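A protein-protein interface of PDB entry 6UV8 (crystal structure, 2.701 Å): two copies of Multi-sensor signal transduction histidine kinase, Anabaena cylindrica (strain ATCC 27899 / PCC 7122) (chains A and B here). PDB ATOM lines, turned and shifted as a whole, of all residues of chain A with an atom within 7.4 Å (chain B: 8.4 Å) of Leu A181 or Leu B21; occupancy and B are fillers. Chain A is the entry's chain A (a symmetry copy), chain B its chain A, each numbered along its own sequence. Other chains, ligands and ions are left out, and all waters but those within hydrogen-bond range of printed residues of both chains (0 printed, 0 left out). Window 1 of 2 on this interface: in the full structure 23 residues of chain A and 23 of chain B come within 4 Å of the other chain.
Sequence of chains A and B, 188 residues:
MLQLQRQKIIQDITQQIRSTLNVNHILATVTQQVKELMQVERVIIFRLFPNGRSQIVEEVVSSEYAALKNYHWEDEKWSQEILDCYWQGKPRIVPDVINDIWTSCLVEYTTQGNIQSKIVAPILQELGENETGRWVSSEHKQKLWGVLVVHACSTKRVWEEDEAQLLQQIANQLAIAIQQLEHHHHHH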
ATOM      1  N   SER A  19      24.341  14.944 -25.706  1.00  0.00           N
ATOM      2  CA  SER A  19      24.814  13.749 -26.396  1.00  0.00           C
ATOM      3  C   SER A  19      23.680  12.760 -26.604  1.00  0.00           C
ATOM      4  O   SER A  19      23.308  12.436 -27.737  1.00  0.00           O
ATOM      5  CB  SER A  19      25.944  13.091 -25.594  1.00  0.00           C
ATOM      6  OG  SER A  19      26.991  12.634 -26.430  1.00  0.00           O
ATOM      7  N   THR A  20      23.106  12.283 -25.505  1.00  0.00           N
ATOM      8  CA  THR A  20      22.100  11.237 -25.589  1.00  0.00           C
ATOM      9  C   THR A  20      20.856  11.703 -26.335  1.00  0.00           C
ATOM     10  O   THR A  20      20.230  10.914 -27.046  1.00  0.00           O
ATOM     11  CB  THR A  20      21.734  10.785 -24.183  1.00  0.00           C
ATOM     12  OG1 THR A  20      21.002  11.833 -23.544  1.00  0.00           O
ATOM     13  CG2 THR A  20      23.001  10.519 -23.380  1.00  0.00           C
ATOM     14  N   LEU A  21      20.503  12.980 -26.217  1.00  0.00           N
ATOM     15  CA  LEU A  21      19.216  13.467 -26.702  1.00  0.00           C
ATOM     16  C   LEU A  21      19.197  13.776 -28.199  1.00  0.00           C
ATOM     17  O   LEU A  21      18.116  13.972 -28.765  1.00  0.00           O
ATOM     18  CB  LEU A  21      18.822  14.711 -25.905  1.00  0.00           C
ATOM     19  CG  LEU A  21      17.443  15.320 -26.110  1.00  0.00           C
ATOM     20  CD1 LEU A  21      16.406  14.225 -26.034  1.00  0.00           C
ATOM     21  CD2 LEU A  21      17.166  16.418 -25.087  1.00  0.00           C
ATOM     22  N   ASN A  22      20.345  13.824 -28.860  1.00  0.00           N
ATOM     23  CA  ASN A  22      20.361  14.108 -30.287  1.00  0.00           C
ATOM     24  C   ASN A  22      20.368  12.800 -31.063  1.00  0.00           C
ATOM     25  O   ASN A  22      21.084  11.860 -30.704  1.00  0.00           O
ATOM     26  CB  ASN A  22      21.557  14.999 -30.654  1.00  0.00           C
ATOM     27  CG  ASN A  22      22.546  14.331 -31.599  1.00  0.00           C
ATOM     28  OD1 ASN A  22      23.437  13.611 -31.161  1.00  0.00           O
ATOM     29  ND2 ASN A  22      22.422  14.609 -32.895  1.00  0.00           N
ATOM     30  N   VAL A  23      19.545  12.750 -32.122  1.00  0.00           N
ATOM     31  CA  VAL A  23      19.276  11.503 -32.841  1.00  0.00           C
ATOM     32  C   VAL A  23      20.549  10.941 -33.445  1.00  0.00           C
ATOM     33  O   VAL A  23      20.817   9.738 -33.354  1.00  0.00           O
ATOM     34  CB  VAL A  23      18.215  11.720 -33.937  1.00  0.00           C
ATOM     35  CG1 VAL A  23      17.579  10.396 -34.322  1.00  0.00           C
ATOM     36  CG2 VAL A  23      17.179  12.745 -33.518  1.00  0.00           C
ATOM     37  N   ASN A  24      21.341  11.804 -34.089  1.00  0.00           N
ATOM     38  CA  ASN A  24      22.484  11.336 -34.868  1.00  0.00           C
ATOM     39  C   ASN A  24      23.471  10.574 -34.004  1.00  0.00           C
ATOM     40  O   ASN A  24      24.068   9.590 -34.455  1.00  0.00           O
ATOM     41  CB  ASN A  24      23.174  12.513 -35.554  1.00  0.00           C
ATOM     42  CG  ASN A  24      22.502  12.897 -36.852  1.00  0.00           C
ATOM     43  OD1 ASN A  24      21.890  13.962 -36.945  1.00  0.00           O
ATOM     44  ND2 ASN A  24      22.607  12.028 -37.867  1.00  0.00           N
ATOM     45  N   HIS A  25      23.653  11.004 -32.757  1.00  0.00           N
ATOM     46  CA  HIS A  25      24.603  10.327 -31.887  1.00  0.00           C
ATOM     47  C   HIS A  25      24.247   8.864 -31.673  1.00  0.00           C
ATOM     48  O   HIS A  25      25.139   8.048 -31.420  1.00  0.00           O
ATOM     49  CB  HIS A  25      24.695  11.042 -30.540  1.00  0.00           C
ATOM     50  CG  HIS A  25      25.505  10.306 -29.529  1.00  0.00           C
ATOM     51  ND1 HIS A  25      24.937   9.474 -28.590  1.00  0.00           N
ATOM     52  CD2 HIS A  25      26.842  10.257 -29.323  1.00  0.00           C
ATOM     53  CE1 HIS A  25      25.891   8.952 -27.838  1.00  0.00           C
ATOM     54  NE2 HIS A  25      27.055   9.410 -28.263  1.00  0.00           N
ATOM     55  N   ILE A  26      22.977   8.504 -31.785  1.00  0.00           N
ATOM     56  CA  ILE A  26      22.609   7.127 -31.491  1.00  0.00           C
ATOM     57  C   ILE A  26      22.415   6.387 -32.805  1.00  0.00           C
ATOM     58  O   ILE A  26      22.628   5.173 -32.881  1.00  0.00           O
ATOM     59  CB  ILE A  26      21.369   7.053 -30.580  1.00  0.00           C
ATOM     60  CG1 ILE A  26      20.083   6.918 -31.394  1.00  0.00           C
ATOM     61  CG2 ILE A  26      21.325   8.267 -29.613  1.00  0.00           C
ATOM     62  CD1 ILE A  26      18.842   7.187 -30.576  1.00  0.00           C
ATOM     63  N   GLN A 173      14.273  -1.092 -33.805  1.00  0.00           N
ATOM     64  CA  GLN A 173      14.645  -0.454 -32.547  1.00  0.00           C
ATOM     65  C   GLN A 173      14.988   1.019 -32.750  1.00  0.00           C
ATOM     66  O   GLN A 173      14.692   1.858 -31.892  1.00  0.00           O
ATOM     67  CB  GLN A 173      15.817  -1.209 -31.917  1.00  0.00           C
ATOM     68  CG  GLN A 173      15.714  -1.319 -30.421  1.00  0.00           C
ATOM     69  CD  GLN A 173      14.390  -1.904 -29.975  1.00  0.00           C
ATOM     70  OE1 GLN A 173      13.818  -2.768 -30.648  1.00  0.00           O
ATOM     71  NE2 GLN A 173      13.888  -1.432 -28.836  1.00  0.00           N
ATOM     72  N   LEU A 174      15.622   1.340 -33.875  1.00  0.00           N
ATOM     73  CA  LEU A 174      15.799   2.734 -34.248  1.00  0.00           C
ATOM     74  C   LEU A 174      14.459   3.432 -34.403  1.00  0.00           C
ATOM     75  O   LEU A 174      14.274   4.541 -33.894  1.00  0.00           O
ATOM     76  CB  LEU A 174      16.599   2.823 -35.544  1.00  0.00           C
ATOM     77  CG  LEU A 174      18.074   2.503 -35.357  1.00  0.00           C
ATOM     78  CD1 LEU A 174      18.829   2.725 -36.642  1.00  0.00           C
ATOM     79  CD2 LEU A 174      18.626   3.377 -34.262  1.00  0.00           C
ATOM     80  N   ALA A 175      13.511   2.792 -35.096  1.00  0.00           N
ATOM     81  CA  ALA A 175      12.204   3.393 -35.324  1.00  0.00           C
ATOM     82  C   ALA A 175      11.651   3.998 -34.047  1.00  0.00           C
ATOM     83  O   ALA A 175      11.147   5.124 -34.044  1.00  0.00           O
ATOM     84  CB  ALA A 175      11.245   2.345 -35.878  1.00  0.00           C
ATOM     85  N   ILE A 176      11.772   3.267 -32.938  1.00  0.00           N
ATOM     86  CA  ILE A 176      11.275   3.751 -31.656  1.00  0.00           C
ATOM     87  C   ILE A 176      12.127   4.904 -31.159  1.00  0.00           C
ATOM     88  O   ILE A 176      11.616   5.863 -30.564  1.00  0.00           O
ATOM     89  CB  ILE A 176      11.244   2.597 -30.638  1.00  0.00           C
ATOM     90  CG1 ILE A 176      10.373   1.453 -31.162  1.00  0.00           C
ATOM     91  CG2 ILE A 176      10.770   3.100 -29.279  1.00  0.00           C
ATOM     92  CD1 ILE A 176      10.800   0.078 -30.681  1.00  0.00           C
ATOM     93  N   ALA A 177      13.440   4.826 -31.382  1.00  0.00           N
ATOM     94  CA  ALA A 177      14.338   5.878 -30.921  1.00  0.00           C
ATOM     95  C   ALA A 177      14.077   7.179 -31.660  1.00  0.00           C
ATOM     96  O   ALA A 177      14.185   8.268 -31.083  1.00  0.00           O
ATOM     97  CB  ALA A 177      15.789   5.445 -31.102  1.00  0.00           C
ATOM     98  N   ILE A 178      13.718   7.087 -32.935  1.00  0.00           N
ATOM     99  CA  ILE A 178      13.568   8.283 -33.751  1.00  0.00           C
ATOM    100  C   ILE A 178      12.228   8.959 -33.495  1.00  0.00           C
ATOM    101  O   ILE A 178      12.153  10.191 -33.433  1.00  0.00           O
ATOM    102  CB  ILE A 178      13.763   7.918 -35.233  1.00  0.00           C
ATOM    103  CG1 ILE A 178      15.250   7.695 -35.523  1.00  0.00           C
ATOM    104  CG2 ILE A 178      13.165   8.982 -36.142  1.00  0.00           C
ATOM    105  CD1 ILE A 178      15.521   6.560 -36.464  1.00  0.00           C
ATOM    106  N   GLN A 179      11.155   8.177 -33.323  1.00  0.00           N
ATOM    107  CA  GLN A 179       9.840   8.765 -33.087  1.00  0.00           C
ATOM    108  C   GLN A 179       9.840   9.684 -31.877  1.00  0.00           C
ATOM    109  O   GLN A 179       9.023  10.610 -31.813  1.00  0.00           O
ATOM    110  CB  GLN A 179       8.784   7.670 -32.909  1.00  0.00           C
ATOM    111  CG  GLN A 179       7.341   8.185 -32.941  1.00  0.00           C
ATOM    112  CD  GLN A 179       6.298   7.072 -33.007  1.00  0.00           C
ATOM    113  OE1 GLN A 179       6.557   5.992 -33.544  1.00  0.00           O
ATOM    114  NE2 GLN A 179       5.108   7.334 -32.456  1.00  0.00           N
ATOM    115  N   GLN A 180      10.751   9.466 -30.931  1.00  0.00           N
ATOM    116  CA  GLN A 180      10.821  10.314 -29.753  1.00  0.00           C
ATOM    117  C   GLN A 180      11.545  11.635 -30.014  1.00  0.00           C
ATOM    118  O   GLN A 180      11.162  12.664 -29.447  1.00  0.00           O
ATOM    119  CB  GLN A 180      11.509   9.550 -28.622  1.00  0.00           C
ATOM    120  CG  GLN A 180      10.599   8.606 -27.836  1.00  0.00           C
ATOM    121  CD  GLN A 180       9.939   9.297 -26.651  1.00  0.00           C
ATOM    122  OE1 GLN A 180       9.160  10.235 -26.824  1.00  0.00           O
ATOM    123  NE2 GLN A 180      10.264   8.847 -25.440  1.00  0.00           N
ATOM    124  N   LEU A 181      12.558  11.642 -30.884  1.00  0.00           N
ATOM    125  CA  LEU A 181      13.584  12.683 -30.901  1.00  0.00           C
ATOM    126  C   LEU A 181      13.444  13.670 -32.067  1.00  0.00           C
ATOM    127  O   LEU A 181      14.451  14.163 -32.588  1.00  0.00           O
ATOM    128  CB  LEU A 181      14.963  12.027 -30.931  1.00  0.00           C
ATOM    129  CG  LEU A 181      15.663  11.630 -29.631  1.00  0.00           C
ATOM    130  CD1 LEU A 181      14.719  10.936 -28.697  1.00  0.00           C
ATOM    131  CD2 LEU A 181      16.850  10.729 -29.924  1.00  0.00           C
ATOM    132  N   GLU A 182      12.213  14.002 -32.463  1.00  0.00           N
ATOM    133  CA  GLU A 182      11.975  14.837 -33.638  1.00  0.00           C
ATOM    134  C   GLU A 182      11.569  16.274 -33.310  1.00  0.00           C
ATOM    135  O   GLU A 182      11.345  17.058 -34.238  1.00  0.00           O
ATOM    136  CB  GLU A 182      10.900  14.198 -34.527  1.00  0.00           C
ATOM    137  CG  GLU A 182      11.279  12.858 -35.155  1.00  0.00           C
ATOM    138  CD  GLU A 182      12.312  12.979 -36.269  1.00  0.00           C
ATOM    139  OE1 GLU A 182      13.463  13.365 -35.972  1.00  0.00           O
ATOM    140  OE2 GLU A 182      11.973  12.686 -37.441  1.00  0.00           O
ATOM    141  N   HIS A 183      11.469  16.634 -32.030  1.00  0.00           N
ATOM    142  CA  HIS A 183      11.044  17.973 -31.595  1.00  0.00           C
ATOM    143  C   HIS A 183       9.614  18.282 -32.049  1.00  0.00           C
ATOM    144  O   HIS A 183       8.965  19.187 -31.523  1.00  0.00           O
ATOM    145  CB  HIS A 183      11.999  19.064 -32.111  1.00  0.00           C
ATOM    146  CG  HIS A 183      13.453  18.766 -31.894  1.00  0.00           C
ATOM    147  ND1 HIS A 183      14.182  17.955 -32.740  1.00  0.00           N
ATOM    148  CD2 HIS A 183      14.318  19.184 -30.937  1.00  0.00           C
ATOM    149  CE1 HIS A 183      15.429  17.879 -32.309  1.00  0.00           C
ATOM    150  NE2 HIS A 183      15.537  18.617 -31.217  1.00  0.00           N
ATOM    151  N   THR B  14      19.789  -2.900 -28.049  1.00  0.00           N
ATOM    152  CA  THR B  14      18.494  -2.560 -27.484  1.00  0.00           C
ATOM    153  C   THR B  14      18.655  -1.953 -26.105  1.00  0.00           C
ATOM    154  O   THR B  14      18.011  -0.951 -25.784  1.00  0.00           O
ATOM    155  CB  THR B  14      17.602  -3.789 -27.408  1.00  0.00           C
ATOM    156  OG1 THR B  14      17.747  -4.553 -28.606  1.00  0.00           O
ATOM    157  CG2 THR B  14      16.151  -3.366 -27.253  1.00  0.00           C
ATOM    158  N   GLN B  15      19.529  -2.540 -25.283  1.00  0.00           N
ATOM    159  CA  GLN B  15      19.708  -2.065 -23.915  1.00  0.00           C
ATOM    160  C   GLN B  15      20.070  -0.587 -23.883  1.00  0.00           C
ATOM    161  O   GLN B  15      19.593   0.155 -23.021  1.00  0.00           O
ATOM    162  CB  GLN B  15      20.786  -2.891 -23.206  1.00  0.00           C
ATOM    163  CG  GLN B  15      20.841  -2.710 -21.696  1.00  0.00           C
ATOM    164  CD  GLN B  15      19.780  -3.518 -20.965  1.00  0.00           C
ATOM    165  OE1 GLN B  15      19.672  -4.735 -21.146  1.00  0.00           O
ATOM    166  NE2 GLN B  15      18.990  -2.844 -20.132  1.00  0.00           N
ATOM    167  N   GLN B  16      20.904  -0.134 -24.820  1.00  0.00           N
ATOM    168  CA  GLN B  16      21.286   1.273 -24.831  1.00  0.00           C
ATOM    169  C   GLN B  16      20.152   2.154 -25.332  1.00  0.00           C
ATOM    170  O   GLN B  16      19.863   3.192 -24.727  1.00  0.00           O
ATOM    171  CB  GLN B  16      22.540   1.480 -25.679  1.00  0.00           C
ATOM    172  CG  GLN B  16      23.791   0.876 -25.054  1.00  0.00           C
ATOM    173  CD  GLN B  16      24.206  -0.423 -25.718  1.00  0.00           C
ATOM    174  OE1 GLN B  16      24.052  -0.583 -26.925  1.00  0.00           O
ATOM    175  NE2 GLN B  16      24.720  -1.368 -24.926  1.00  0.00           N
ATOM    176  N   ILE B  17      19.500   1.758 -26.428  1.00  0.00           N
ATOM    177  CA  ILE B  17      18.367   2.525 -26.941  1.00  0.00           C
ATOM    178  C   ILE B  17      17.331   2.737 -25.848  1.00  0.00           C
ATOM    179  O   ILE B  17      16.858   3.854 -25.629  1.00  0.00           O
ATOM    180  CB  ILE B  17      17.753   1.827 -28.165  1.00  0.00           C
ATOM    181  CG1 ILE B  17      18.720   1.888 -29.340  1.00  0.00           C
ATOM    182  CG2 ILE B  17      16.436   2.467 -28.542  1.00  0.00           C
ATOM    183  CD1 ILE B  17      18.154   1.319 -30.604  1.00  0.00           C
ATOM    184  N   ARG B  18      16.972   1.669 -25.137  1.00  0.00           N
ATOM    185  CA  ARG B  18      16.005   1.806 -24.054  1.00  0.00           C
ATOM    186  C   ARG B  18      16.582   2.621 -22.907  1.00  0.00           C
ATOM    187  O   ARG B  18      15.891   3.469 -22.331  1.00  0.00           O
ATOM    188  CB  ARG B  18      15.563   0.425 -23.569  1.00  0.00           C
ATOM    189  CG  ARG B  18      15.246  -0.549 -24.696  1.00  0.00           C
ATOM    190  CD  ARG B  18      13.757  -0.698 -24.930  1.00  0.00           C
ATOM    191  NE  ARG B  18      13.151  -1.593 -23.950  1.00  0.00           N
ATOM    192  CZ  ARG B  18      13.019  -2.906 -24.123  1.00  0.00           C
ATOM    193  NH1 ARG B  18      12.455  -3.646 -23.175  1.00  0.00           N
ATOM    194  NH2 ARG B  18      13.444  -3.483 -25.243  1.00  0.00           N
ATOM    195  N   SER B  19      17.853   2.382 -22.574  1.00  0.00           N
ATOM    196  CA  SER B  19      18.505   3.097 -21.481  1.00  0.00           C
ATOM    197  C   SER B  19      18.440   4.598 -21.702  1.00  0.00           C
ATOM    198  O   SER B  19      17.837   5.339 -20.918  1.00  0.00           O
ATOM    199  CB  SER B  19      19.966   2.647 -21.357  1.00  0.00           C
ATOM    200  OG  SER B  19      20.359   2.488 -20.006  1.00  0.00           O
ATOM    201  N   THR B  20      19.048   5.060 -22.789  1.00  0.00           N
ATOM    202  CA  THR B  20      19.155   6.490 -23.026  1.00  0.00           C
ATOM    203  C   THR B  20      17.790   7.139 -23.214  1.00  0.00           C
ATOM    204  O   THR B  20      17.586   8.283 -22.799  1.00  0.00           O
ATOM    205  CB  THR B  20      20.025   6.727 -24.253  1.00  0.00           C
ATOM    206  OG1 THR B  20      19.305   6.300 -25.410  1.00  0.00           O
ATOM    207  CG2 THR B  20      21.304   5.905 -24.145  1.00  0.00           C
ATOM    208  N   LEU B  21      16.835   6.420 -23.799  1.00  0.00           N
ATOM    209  CA  LEU B  21      15.577   7.022 -24.225  1.00  0.00           C
ATOM    210  C   LEU B  21      14.548   7.160 -23.103  1.00  0.00           C
ATOM    211  O   LEU B  21      13.541   7.856 -23.283  1.00  0.00           O
ATOM    212  CB  LEU B  21      14.993   6.196 -25.372  1.00  0.00           C
ATOM    213  CG  LEU B  21      13.757   6.703 -26.101  1.00  0.00           C
ATOM    214  CD1 LEU B  21      13.968   8.151 -26.473  1.00  0.00           C
ATOM    215  CD2 LEU B  21      13.455   5.853 -27.332  1.00  0.00           C
ATOM    216  N   ASN B  22      14.760   6.531 -21.955  1.00  0.00           N
ATOM    217  CA  ASN B  22      13.803   6.649 -20.865  1.00  0.00           C
ATOM    218  C   ASN B  22      14.237   7.769 -19.931  1.00  0.00           C
ATOM    219  O   ASN B  22      15.422   7.896 -19.610  1.00  0.00           O
ATOM    220  CB  ASN B  22      13.652   5.311 -20.124  1.00  0.00           C
ATOM    221  CG  ASN B  22      14.092   5.369 -18.667  1.00  0.00           C
ATOM    222  OD1 ASN B  22      15.269   5.205 -18.367  1.00  0.00           O
ATOM    223  ND2 ASN B  22      13.138   5.552 -17.757  1.00  0.00           N
ATOM    224  N   VAL B  23      13.258   8.588 -19.517  1.00  0.00           N
ATOM    225  CA  VAL B  23      13.537   9.831 -18.794  1.00  0.00           C
ATOM    226  C   VAL B  23      14.244   9.547 -17.482  1.00  0.00           C
ATOM    227  O   VAL B  23      15.219  10.219 -17.128  1.00  0.00           O
ATOM    228  CB  VAL B  23      12.239  10.623 -18.541  1.00  0.00           C
ATOM    229  CG1 VAL B  23      12.558  12.082 -18.270  1.00  0.00           C
ATOM    230  CG2 VAL B  23      11.255  10.461 -19.683  1.00  0.00           C
ATOM    231  N   ASN B  24      13.747   8.559 -16.732  1.00  0.00           N
ATOM    232  CA  ASN B  24      14.227   8.332 -15.373  1.00  0.00           C
ATOM    233  C   ASN B  24      15.716   8.037 -15.351  1.00  0.00           C
ATOM    234  O   ASN B  24      16.426   8.463 -14.433  1.00  0.00           O
ATOM    235  CB  ASN B  24      13.449   7.194 -14.718  1.00  0.00           C
ATOM    236  CG  ASN B  24      12.136   7.657 -14.130  1.00  0.00           C
ATOM    237  OD1 ASN B  24      11.069   7.310 -14.638  1.00  0.00           O
ATOM    238  ND2 ASN B  24      12.204   8.453 -13.053  1.00  0.00           N
ATOM    239  N   HIS B  25      16.211   7.317 -16.356  1.00  0.00           N
ATOM    240  CA  HIS B  25      17.628   6.984 -16.379  1.00  0.00           C
ATOM    241  C   HIS B  25      18.511   8.221 -16.405  1.00  0.00           C
ATOM    242  O   HIS B  25      19.651   8.169 -15.931  1.00  0.00           O
ATOM    243  CB  HIS B  25      17.945   6.093 -17.581  1.00  0.00           C
ATOM    244  CG  HIS B  25      19.404   5.860 -17.780  1.00  0.00           C
ATOM    245  ND1 HIS B  25      20.160   6.612 -18.652  1.00  0.00           N
ATOM    246  CD2 HIS B  25      20.251   4.976 -17.205  1.00  0.00           C
ATOM    247  CE1 HIS B  25      21.412   6.191 -18.614  1.00  0.00           C
ATOM    248  NE2 HIS B  25      21.494   5.200 -17.744  1.00  0.00           N
ATOM    249  N   ILE B  26      18.017   9.335 -16.924  1.00  0.00           N
ATOM    250  CA  ILE B  26      18.881  10.499 -17.040  1.00  0.00           C
ATOM    251  C   ILE B  26      18.545  11.467 -15.916  1.00  0.00           C
ATOM    252  O   ILE B  26      19.407  12.221 -15.456  1.00  0.00           O
ATOM    253  CB  ILE B  26      18.775  11.149 -18.433  1.00  0.00           C
ATOM    254  CG1 ILE B  26      17.741  12.275 -18.449  1.00  0.00           C
ATOM    255  CG2 ILE B  26      18.488  10.076 -19.518  1.00  0.00           C
ATOM    256  CD1 ILE B  26      17.360  12.700 -19.847  1.00  0.00           C
ATOM    257  N   ALA B 177      15.618  18.113 -21.596  1.00  0.00           N
ATOM    258  CA  ALA B 177      15.655  16.661 -21.723  1.00  0.00           C
ATOM    259  C   ALA B 177      14.267  16.065 -21.574  1.00  0.00           C
ATOM    260  O   ALA B 177      13.928  15.075 -22.233  1.00  0.00           O
ATOM    261  CB  ALA B 177      16.602  16.069 -20.683  1.00  0.00           C
ATOM    262  N   GLN B 180      11.423  16.414 -24.508  1.00  0.00           N
ATOM    263  CA  GLN B 180      11.550  15.482 -25.617  1.00  0.00           C
ATOM    264  C   GLN B 180      10.927  14.118 -25.319  1.00  0.00           C
ATOM    265  O   GLN B 180      10.364  13.494 -26.225  1.00  0.00           O
ATOM    266  CB  GLN B 180      13.028  15.321 -25.973  1.00  0.00           C
ATOM    267  CG  GLN B 180      13.594  16.412 -26.882  1.00  0.00           C
ATOM    268  CD  GLN B 180      13.442  16.068 -28.357  1.00  0.00           C
ATOM    269  OE1 GLN B 180      12.326  15.940 -28.862  1.00  0.00           O
ATOM    270  NE2 GLN B 180      14.568  15.897 -29.050  1.00  0.00           N
ATOM    271  N   LEU B 181      10.981  13.655 -24.068  1.00  0.00           N
ATOM    272  CA  LEU B 181      10.832  12.240 -23.737  1.00  0.00           C
ATOM    273  C   LEU B 181       9.479  11.890 -23.105  1.00  0.00           C
ATOM    274  O   LEU B 181       9.402  11.000 -22.252  1.00  0.00           O
ATOM    275  CB  LEU B 181      11.969  11.821 -22.807  1.00  0.00           C
ATOM    276  CG  LEU B 181      13.306  11.347 -23.379  1.00  0.00           C
ATOM    277  CD1 LEU B 181      13.772  12.245 -24.484  1.00  0.00           C
ATOM    278  CD2 LEU B 181      14.358  11.292 -22.285  1.00  0.00           C
ATOM    279  N   GLU B 182       8.398  12.546 -23.536  1.00  0.00           N
ATOM    280  CA  GLU B 182       7.087  12.373 -22.915  1.00  0.00           C
ATOM    281  C   GLU B 182       6.115  11.525 -23.736  1.00  0.00           C
ATOM    282  O   GLU B 182       4.980  11.321 -23.294  1.00  0.00           O
ATOM    283  CB  GLU B 182       6.453  13.742 -22.638  1.00  0.00           C
ATOM    284  CG  GLU B 182       7.183  14.609 -21.613  1.00  0.00           C
ATOM    285  CD  GLU B 182       7.040  14.108 -20.181  1.00  0.00           C
ATOM    286  OE1 GLU B 182       7.556  13.008 -19.881  1.00  0.00           O
ATOM    287  OE2 GLU B 182       6.413  14.813 -19.354  1.00  0.00           O
ATOM    288  N   HIS B 183       6.526  11.032 -24.904  1.00  0.00           N
ATOM    289  CA  HIS B 183       5.668  10.242 -25.799  1.00  0.00           C
ATOM    290  C   HIS B 183       4.466  11.057 -26.286  1.00  0.00           C
ATOM    291  O   HIS B 183       3.821  10.705 -27.275  1.00  0.00           O
ATOM    292  CB  HIS B 183       5.177   8.952 -25.116  1.00  0.00           C
ATOM    293  CG  HIS B 183       6.254   8.168 -24.428  1.00  0.00           C
ATOM    294  ND1 HIS B 183       6.705   8.476 -23.160  1.00  0.00           N
ATOM    295  CD2 HIS B 183       6.959   7.080 -24.823  1.00  0.00           C
ATOM    296  CE1 HIS B 183       7.646   7.616 -22.809  1.00  0.00           C
ATOM    297  NE2 HIS B 183       7.817   6.759 -23.801  1.00  0.00           N
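The backbone carbonyl oxygen (O) of Ile B17 sits at hydrogen-bond distance from the side-chain hydroxyl (OG1) of Thr B20 (3.5 Å).
Leu A21 touches Gln B180, and with the chains exchanged Gln A180 touches Leu B21.
Gln A180 touches its own counterpart, Gln B180.
Gln A180 touches Leu B181, and with the chains exchanged Leu A181 touches Gln B180.
Gln A180 touches His B183, and with the chains exchanged His A183 touches Gln B180.
13 positions are printed for both chains.
Ala B177 touches Leu A21 (CA to CD2, 3.7 Å).
Gln B180 touches Leu A21 (CB to CD1, 3.6 Å).
Leu A21 touches Leu B181.
Thr B14 touches Gln A173.
CD1 of Ile B17 touches CG of Gln A173, at 3.6 Å.
Leu B21 touches Ile A176.
CB of Ala A177 touches CG2 of Ile B17, 3.98 Å away.
CB of Gln A180 touches CD1 of Leu B21, 3.6 Å away.
Leu B181 touches Gln A180.
CA of Leu A181 touches NE2 of Gln B180, 3.8 Å away.
Printed residues of chain A within 4 Å of Leu B21: Ile A176, Ala A177, Gln A180 and Leu A181.
Printed residues of chain B within 4 Å of His A183: Gln B180 (3.4 Å).
Of the printed residues of chain A, Gln B180 touches Leu A21 (3.6 Å), Gln A180 (3.4 Å), Leu A181 (3.8 Å) and His A183 (3.4 Å).
The nearest residue of chain A that does not touch Leu B21 is Ile A178 (5.7 Å).
The backbone carbonyl oxygen (O) of Gln B180 sits close to the backbone carbonyl oxygen (O) of Gln A180, at 3.4 Å.
The backbone NH (N) of His B183 sits at hydrogen-bond distance from the side-chain amide oxygen (OE1) of Gln A180.
N of His A183 sits at hydrogen-bond distance from OE1 of Gln B180, 3.4 Å away.
Hydrophobic or aromatic side chains of chain B that line the printed part of chain A: Ile B17, Leu B21, Leu B181 and His B183.
Of the 19 printed residues of chain A, 7 touch a printed residue of chain B.
Hydrophobic or aromatic side chains of chain A that line the printed part of chain B: Leu A21, Ala A177, Leu A181 and His A183.
Among the printed residues, 16 pairs touch across the chains.
Among the printed residues, no Asp or Glu carboxylate lies within 4 Å of a Lys or Arg side-chain nitrogen of the other chain.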
